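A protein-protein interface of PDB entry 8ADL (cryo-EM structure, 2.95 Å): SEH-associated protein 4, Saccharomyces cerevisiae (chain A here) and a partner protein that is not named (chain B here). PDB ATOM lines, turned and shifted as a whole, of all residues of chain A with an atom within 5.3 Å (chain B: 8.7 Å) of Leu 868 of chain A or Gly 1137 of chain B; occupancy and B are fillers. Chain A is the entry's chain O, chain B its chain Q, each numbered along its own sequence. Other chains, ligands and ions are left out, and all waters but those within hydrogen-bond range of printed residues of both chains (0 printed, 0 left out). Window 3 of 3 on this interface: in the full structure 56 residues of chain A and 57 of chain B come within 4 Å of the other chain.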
ATOM      1  N   ASP A 854      26.109 -10.663  30.392  1.00  0.00           N
ATOM      2  CA  ASP A 854      25.636 -10.886  29.026  1.00  0.00           C
ATOM      3  C   ASP A 854      26.715 -10.562  27.995  1.00  0.00           C
ATOM      4  O   ASP A 854      26.896 -11.311  27.023  1.00  0.00           O
ATOM      5  CB  ASP A 854      24.378 -10.061  28.765  1.00  0.00           C
ATOM      6  CG  ASP A 854      23.116 -10.767  29.218  1.00  0.00           C
ATOM      7  OD1 ASP A 854      23.064 -12.011  29.128  1.00  0.00           O
ATOM      8  OD2 ASP A 854      22.174 -10.077  29.661  1.00  0.00           O
ATOM      9  N   VAL A 855      27.448  -9.461  28.188  1.00  0.00           N
ATOM     10  CA  VAL A 855      28.509  -9.139  27.233  1.00  0.00           C
ATOM     11  C   VAL A 855      29.671 -10.122  27.368  1.00  0.00           C
ATOM     12  O   VAL A 855      30.350 -10.421  26.379  1.00  0.00           O
ATOM     13  CB  VAL A 855      28.962  -7.666  27.344  1.00  0.00           C
ATOM     14  CG1 VAL A 855      27.770  -6.733  27.205  1.00  0.00           C
ATOM     15  CG2 VAL A 855      29.712  -7.387  28.632  1.00  0.00           C
ATOM     16  N   ARG A 857      29.190 -13.326  28.104  1.00  0.00           N
ATOM     17  CA  ARG A 857      28.669 -14.478  27.371  1.00  0.00           C
ATOM     18  C   ARG A 857      28.852 -14.299  25.872  1.00  0.00           C
ATOM     19  O   ARG A 857      29.225 -15.244  25.168  1.00  0.00           O
ATOM     20  CB  ARG A 857      27.188 -14.691  27.683  1.00  0.00           C
ATOM     21  CG  ARG A 857      26.885 -15.257  29.046  1.00  0.00           C
ATOM     22  CD  ARG A 857      25.389 -15.264  29.293  1.00  0.00           C
ATOM     23  NE  ARG A 857      24.654 -15.705  28.114  1.00  0.00           N
ATOM     24  CZ  ARG A 857      23.444 -15.278  27.784  1.00  0.00           C
ATOM     25  NH1 ARG A 857      22.798 -14.390  28.522  1.00  0.00           N
ATOM     26  NH2 ARG A 857      22.867 -15.752  26.683  1.00  0.00           N
ATOM     27  N   SER A 858      28.574 -13.096  25.368  1.00  0.00           N
ATOM     28  CA  SER A 858      28.752 -12.833  23.943  1.00  0.00           C
ATOM     29  C   SER A 858      30.223 -12.868  23.542  1.00  0.00           C
ATOM     30  O   SER A 858      30.555 -13.295  22.429  1.00  0.00           O
ATOM     31  CB  SER A 858      28.126 -11.489  23.579  1.00  0.00           C
ATOM     32  OG  SER A 858      26.723 -11.533  23.757  1.00  0.00           O
ATOM     33  N   SER A 861      31.159 -16.669  23.547  1.00  0.00           N
ATOM     34  CA  SER A 861      30.480 -17.524  22.585  1.00  0.00           C
ATOM     35  C   SER A 861      31.043 -17.396  21.176  1.00  0.00           C
ATOM     36  O   SER A 861      30.536 -18.051  20.261  1.00  0.00           O
ATOM     37  CB  SER A 861      28.980 -17.216  22.565  1.00  0.00           C
ATOM     38  OG  SER A 861      28.469 -17.098  23.880  1.00  0.00           O
ATOM     39  N   ARG A 862      32.067 -16.567  20.978  1.00  0.00           N
ATOM     40  CA  ARG A 862      32.648 -16.403  19.654  1.00  0.00           C
ATOM     41  C   ARG A 862      33.508 -17.609  19.298  1.00  0.00           C
ATOM     42  O   ARG A 862      34.362 -18.030  20.084  1.00  0.00           O
ATOM     43  CB  ARG A 862      33.465 -15.115  19.586  1.00  0.00           C
ATOM     44  CG  ARG A 862      32.643 -13.872  19.873  1.00  0.00           C
ATOM     45  CD  ARG A 862      31.665 -13.604  18.737  1.00  0.00           C
ATOM     46  NE  ARG A 862      30.822 -12.442  18.991  1.00  0.00           N
ATOM     47  CZ  ARG A 862      31.139 -11.199  18.659  1.00  0.00           C
ATOM     48  NH1 ARG A 862      32.280 -10.915  18.053  1.00  0.00           N
ATOM     49  NH2 ARG A 862      30.288 -10.216  18.940  1.00  0.00           N
ATOM     50  N   GLY A 866      34.670 -16.573  14.362  1.00  0.00           N
ATOM     51  CA  GLY A 866      34.158 -15.305  14.857  1.00  0.00           C
ATOM     52  C   GLY A 866      32.647 -15.211  14.896  1.00  0.00           C
ATOM     53  O   GLY A 866      32.120 -14.168  15.310  1.00  0.00           O
ATOM     54  N   VAL A 867      31.928 -16.254  14.484  1.00  0.00           N
ATOM     55  CA  VAL A 867      30.472 -16.217  14.452  1.00  0.00           C
ATOM     56  C   VAL A 867      29.923 -16.336  15.866  1.00  0.00           C
ATOM     57  O   VAL A 867      30.260 -17.270  16.606  1.00  0.00           O
ATOM     58  CB  VAL A 867      29.926 -17.332  13.548  1.00  0.00           C
ATOM     59  CG1 VAL A 867      28.446 -17.113  13.277  1.00  0.00           C
ATOM     60  CG2 VAL A 867      30.709 -17.390  12.246  1.00  0.00           C
ATOM     61  N   LEU A 868      29.075 -15.385  16.250  1.00  0.00           N
ATOM     62  CA  LEU A 868      28.487 -15.372  17.583  1.00  0.00           C
ATOM     63  C   LEU A 868      27.373 -16.409  17.647  1.00  0.00           C
ATOM     64  O   LEU A 868      26.371 -16.299  16.934  1.00  0.00           O
ATOM     65  CB  LEU A 868      27.952 -13.982  17.916  1.00  0.00           C
ATOM     66  CG  LEU A 868      27.179 -13.835  19.228  1.00  0.00           C
ATOM     67  CD1 LEU A 868      28.052 -14.212  20.413  1.00  0.00           C
ATOM     68  CD2 LEU A 868      26.646 -12.417  19.380  1.00  0.00           C
ATOM     69  N   THR A 869      27.552 -17.415  18.499  1.00  0.00           N
ATOM     70  CA  THR A 869      26.588 -18.494  18.660  1.00  0.00           C
ATOM     71  C   THR A 869      25.611 -18.269  19.805  1.00  0.00           C
ATOM     72  O   THR A 869      24.786 -19.147  20.074  1.00  0.00           O
ATOM     73  CB  THR A 869      27.316 -19.825  18.867  1.00  0.00           C
ATOM     74  OG1 THR A 869      28.141 -19.744  20.036  1.00  0.00           O
ATOM     75  CG2 THR A 869      28.181 -20.151  17.661  1.00  0.00           C
ATOM     76  N   ALA A 870      25.679 -17.128  20.485  1.00  0.00           N
ATOM     77  CA  ALA A 870      24.757 -16.880  21.580  1.00  0.00           C
ATOM     78  C   ALA A 870      23.403 -16.425  21.046  1.00  0.00           C
ATOM     79  O   ALA A 870      23.266 -16.000  19.896  1.00  0.00           O
ATOM     80  CB  ALA A 870      25.326 -15.833  22.537  1.00  0.00           C
ATOM     81  N   ILE A 872      20.616 -13.761  21.004  1.00  0.00           N
ATOM     82  CA  ILE A 872      20.435 -12.340  21.258  1.00  0.00           C
ATOM     83  C   ILE A 872      18.970 -11.965  21.068  1.00  0.00           C
ATOM     84  O   ILE A 872      18.186 -12.681  20.438  1.00  0.00           O
ATOM     85  CB  ILE A 872      21.339 -11.482  20.350  1.00  0.00           C
ATOM     86  CG1 ILE A 872      20.956 -11.677  18.881  1.00  0.00           C
ATOM     87  CG2 ILE A 872      22.800 -11.833  20.576  1.00  0.00           C
ATOM     88  CD1 ILE A 872      21.614 -10.691  17.942  1.00  0.00           C
ATOM     89  N   ASN B1099      16.822  -3.053  27.561  1.00  0.00           N
ATOM     90  CA  ASN B1099      17.871  -4.062  27.514  1.00  0.00           C
ATOM     91  C   ASN B1099      18.827  -3.982  28.697  1.00  0.00           C
ATOM     92  O   ASN B1099      19.786  -4.758  28.753  1.00  0.00           O
ATOM     93  CB  ASN B1099      18.649  -3.942  26.204  1.00  0.00           C
ATOM     94  CG  ASN B1099      17.836  -4.392  25.012  1.00  0.00           C
ATOM     95  OD1 ASN B1099      17.746  -5.583  24.724  1.00  0.00           O
ATOM     96  ND2 ASN B1099      17.223  -3.440  24.321  1.00  0.00           N
ATOM     97  N   CYS B1115      22.289  -1.783  15.765  1.00  0.00           N
ATOM     98  CA  CYS B1115      21.391  -2.720  16.422  1.00  0.00           C
ATOM     99  C   CYS B1115      20.134  -1.980  16.856  1.00  0.00           C
ATOM    100  O   CYS B1115      20.195  -0.828  17.292  1.00  0.00           O
ATOM    101  CB  CYS B1115      22.063  -3.397  17.622  1.00  0.00           C
ATOM    102  SG  CYS B1115      22.249  -2.395  19.112  1.00  0.00           S
ATOM    103  N   HIS B1117      17.831  -1.774  19.312  1.00  0.00           N
ATOM    104  CA  HIS B1117      17.555  -2.084  20.707  1.00  0.00           C
ATOM    105  C   HIS B1117      17.293  -0.807  21.494  1.00  0.00           C
ATOM    106  O   HIS B1117      17.992   0.195  21.321  1.00  0.00           O
ATOM    107  CB  HIS B1117      18.720  -2.854  21.347  1.00  0.00           C
ATOM    108  CG  HIS B1117      18.911  -4.232  20.795  1.00  0.00           C
ATOM    109  ND1 HIS B1117      20.155  -4.808  20.647  1.00  0.00           N
ATOM    110  CD2 HIS B1117      18.016  -5.153  20.364  1.00  0.00           C
ATOM    111  CE1 HIS B1117      20.018  -6.021  20.144  1.00  0.00           C
ATOM    112  NE2 HIS B1117      18.730  -6.255  19.963  1.00  0.00           N
ATOM    113  N   TRP B1127      24.623   2.925  31.978  1.00  0.00           N
ATOM    114  CA  TRP B1127      25.379   1.836  31.364  1.00  0.00           C
ATOM    115  C   TRP B1127      26.593   2.341  30.592  1.00  0.00           C
ATOM    116  O   TRP B1127      27.647   1.696  30.604  1.00  0.00           O
ATOM    117  CB  TRP B1127      24.469   1.005  30.457  1.00  0.00           C
ATOM    118  CG  TRP B1127      25.177  -0.085  29.683  1.00  0.00           C
ATOM    119  CD1 TRP B1127      25.161  -0.259  28.331  1.00  0.00           C
ATOM    120  CD2 TRP B1127      25.997  -1.144  30.210  1.00  0.00           C
ATOM    121  NE1 TRP B1127      25.915  -1.351  27.981  1.00  0.00           N
ATOM    122  CE2 TRP B1127      26.438  -1.912  29.115  1.00  0.00           C
ATOM    123  CE3 TRP B1127      26.398  -1.516  31.499  1.00  0.00           C
ATOM    124  CZ2 TRP B1127      27.261  -3.025  29.267  1.00  0.00           C
ATOM    125  CZ3 TRP B1127      27.217  -2.619  31.646  1.00  0.00           C
ATOM    126  CH2 TRP B1127      27.638  -3.361  30.537  1.00  0.00           C
ATOM    127  N   GLU B1133      29.662  -2.142  24.964  1.00  0.00           N
ATOM    128  CA  GLU B1133      28.829  -2.799  23.967  1.00  0.00           C
ATOM    129  C   GLU B1133      27.368  -2.720  24.396  1.00  0.00           C
ATOM    130  O   GLU B1133      27.040  -2.203  25.466  1.00  0.00           O
ATOM    131  CB  GLU B1133      29.260  -4.255  23.768  1.00  0.00           C
ATOM    132  CG  GLU B1133      30.678  -4.420  23.252  1.00  0.00           C
ATOM    133  CD  GLU B1133      31.033  -5.869  22.986  1.00  0.00           C
ATOM    134  OE1 GLU B1133      30.224  -6.754  23.338  1.00  0.00           O
ATOM    135  OE2 GLU B1133      32.119  -6.123  22.425  1.00  0.00           O
ATOM    136  N   CYS B1134      26.494  -3.251  23.548  1.00  0.00           N
ATOM    137  CA  CYS B1134      25.072  -3.276  23.857  1.00  0.00           C
ATOM    138  C   CYS B1134      24.816  -4.202  25.046  1.00  0.00           C
ATOM    139  O   CYS B1134      25.388  -5.295  25.116  1.00  0.00           O
ATOM    140  CB  CYS B1134      24.273  -3.739  22.637  1.00  0.00           C
ATOM    141  SG  CYS B1134      22.477  -3.604  22.781  1.00  0.00           S
ATOM    142  N   PRO B1135      23.982  -3.784  26.007  1.00  0.00           N
ATOM    143  CA  PRO B1135      23.728  -4.635  27.183  1.00  0.00           C
ATOM    144  C   PRO B1135      22.983  -5.921  26.872  1.00  0.00           C
ATOM    145  O   PRO B1135      22.990  -6.832  27.708  1.00  0.00           O
ATOM    146  CB  PRO B1135      22.905  -3.726  28.105  1.00  0.00           C
ATOM    147  CG  PRO B1135      22.318  -2.699  27.204  1.00  0.00           C
ATOM    148  CD  PRO B1135      23.321  -2.475  26.120  1.00  0.00           C
ATOM    149  N   SER B1136      22.341  -6.030  25.708  1.00  0.00           N
ATOM    150  CA  SER B1136      21.749  -7.292  25.292  1.00  0.00           C
ATOM    151  C   SER B1136      22.780  -8.271  24.746  1.00  0.00           C
ATOM    152  O   SER B1136      22.430  -9.421  24.464  1.00  0.00           O
ATOM    153  CB  SER B1136      20.668  -7.049  24.236  1.00  0.00           C
ATOM    154  OG  SER B1136      21.165  -6.253  23.173  1.00  0.00           O
ATOM    155  N   GLY B1137      24.029  -7.843  24.599  1.00  0.00           N
ATOM    156  CA  GLY B1137      25.096  -8.706  24.128  1.00  0.00           C
ATOM    157  C   GLY B1137      24.986  -9.126  22.679  1.00  0.00           C
ATOM    158  O   GLY B1137      25.244 -10.292  22.356  1.00  0.00           O
ATOM    159  N   CYS B1138      24.607  -8.208  21.796  1.00  0.00           N
ATOM    160  CA  CYS B1138      24.587  -8.481  20.367  1.00  0.00           C
ATOM    161  C   CYS B1138      25.915  -8.174  19.688  1.00  0.00           C
ATOM    162  O   CYS B1138      26.057  -8.443  18.491  1.00  0.00           O
ATOM    163  CB  CYS B1138      23.467  -7.687  19.688  1.00  0.00           C
ATOM    164  SG  CYS B1138      23.568  -5.900  19.931  1.00  0.00           S
ATOM    165  N   GLY B1139      26.885  -7.623  20.415  1.00  0.00           N
ATOM    166  CA  GLY B1139      28.176  -7.325  19.829  1.00  0.00           C
ATOM    167  C   GLY B1139      28.263  -6.009  19.094  1.00  0.00           C
ATOM    168  O   GLY B1139      29.197  -5.812  18.311  1.00  0.00           O
ATOM    169  N   CYS B1140      27.319  -5.100  19.318  1.00  0.00           N
ATOM    170  CA  CYS B1140      27.279  -3.816  18.631  1.00  0.00           C
ATOM    171  C   CYS B1140      27.892  -2.740  19.520  1.00  0.00           C
ATOM    172  O   CYS B1140      27.423  -2.514  20.641  1.00  0.00           O
ATOM    173  CB  CYS B1140      25.847  -3.443  18.253  1.00  0.00           C
ATOM    174  SG  CYS B1140      25.678  -1.769  17.596  1.00  0.00           S
ATOM    175  N   CYS B1142      27.678   0.369  20.366  1.00  0.00           N
ATOM    176  CA  CYS B1142      26.702   1.451  20.261  1.00  0.00           C
ATOM    177  C   CYS B1142      27.240   2.876  20.435  1.00  0.00           C
ATOM    178  O   CYS B1142      26.643   3.784  19.831  1.00  0.00           O
ATOM    179  CB  CYS B1142      25.574   1.204  21.270  1.00  0.00           C
ATOM    180  SG  CYS B1142      24.556  -0.237  20.940  1.00  0.00           S
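The backbone carbonyl oxygen (O) of Gly 1137 of chain B sits close to the side-chain hydroxyl (OG) of Ser 858 of chain A, at 2.4 Å.
The side-chain hydroxyl of Ser 1136 of chain B sits close to the side-chain sulfur of Cys 1134 of chain B (3.0 Å). The backbone NH of Cys 1134 of chain B sits at hydrogen-bond distance from the backbone carbonyl oxygen of Cys 1140 of chain B. NH1 of Arg 857 of chain A lies within salt-bridge range of OD1 of Asp 854 of chain A, at 2.5 Å. The backbone carbonyl oxygen of Asp 854 of chain A is in hydrogen-bond range of the side-chain hydroxyl of Ser 858 of chain A (3.3 Å).
Pro 1135 of chain B touches Asp 854 of chain A. Cys 1134 of chain B touches Val 855 of chain A (O to CG1, 3.5 Å). Arg 862 of chain A touches Gly 1139 of chain B (NH2 to CA, 3.7 Å). O of Gly 1137 of chain B touches CD2 of Leu 868 of chain A, 3.9 Å away. Ile 872 of chain A touches Gly 1137 of chain B (CG2 to O, 3.4 Å). CA of Cys 1138 of chain B touches CG2 of Ile 872 of chain A (3.8 Å).
Of the printed residues of chain B, Val 855 of chain A touches Cys 1134. Of chain B, only Gly 1137 comes within 4 Å of Leu 868 of chain A. No residue of chain B comes within 4 Å of Thr 869 of chain A. Printed residues of chain B within 4 Å of Ile 872 of chain A: Gly 1137 and Cys 1138. Glu 1133 of chain B touches none of the printed residues of chain A. Printed residues of chain A within 4 Å of Cys 1134 of chain B: Val 855. Gly 1137 of chain B touches just these residues of chain A: Ser 858 (2.4 Å), Leu 868 (3.9 Å) and Ile 872 (3.4 Å). Printed residues of chain A within 4 Å of Cys 1138 of chain B: Ile 872 (3.8 Å). The nearest residue of chain B that does not touch Leu 868 of chain A is Cys 1138 of chain B (4.1 Å).
Of the 12 printed residues of chain A, 6 touch a printed residue of chain B. Among the printed residues, 7 pairs touch across the chains. Among the printed residues, no Asp or Glu carboxylate lies within 4 Å of a Lys or Arg side-chain nitrogen of the other chain.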
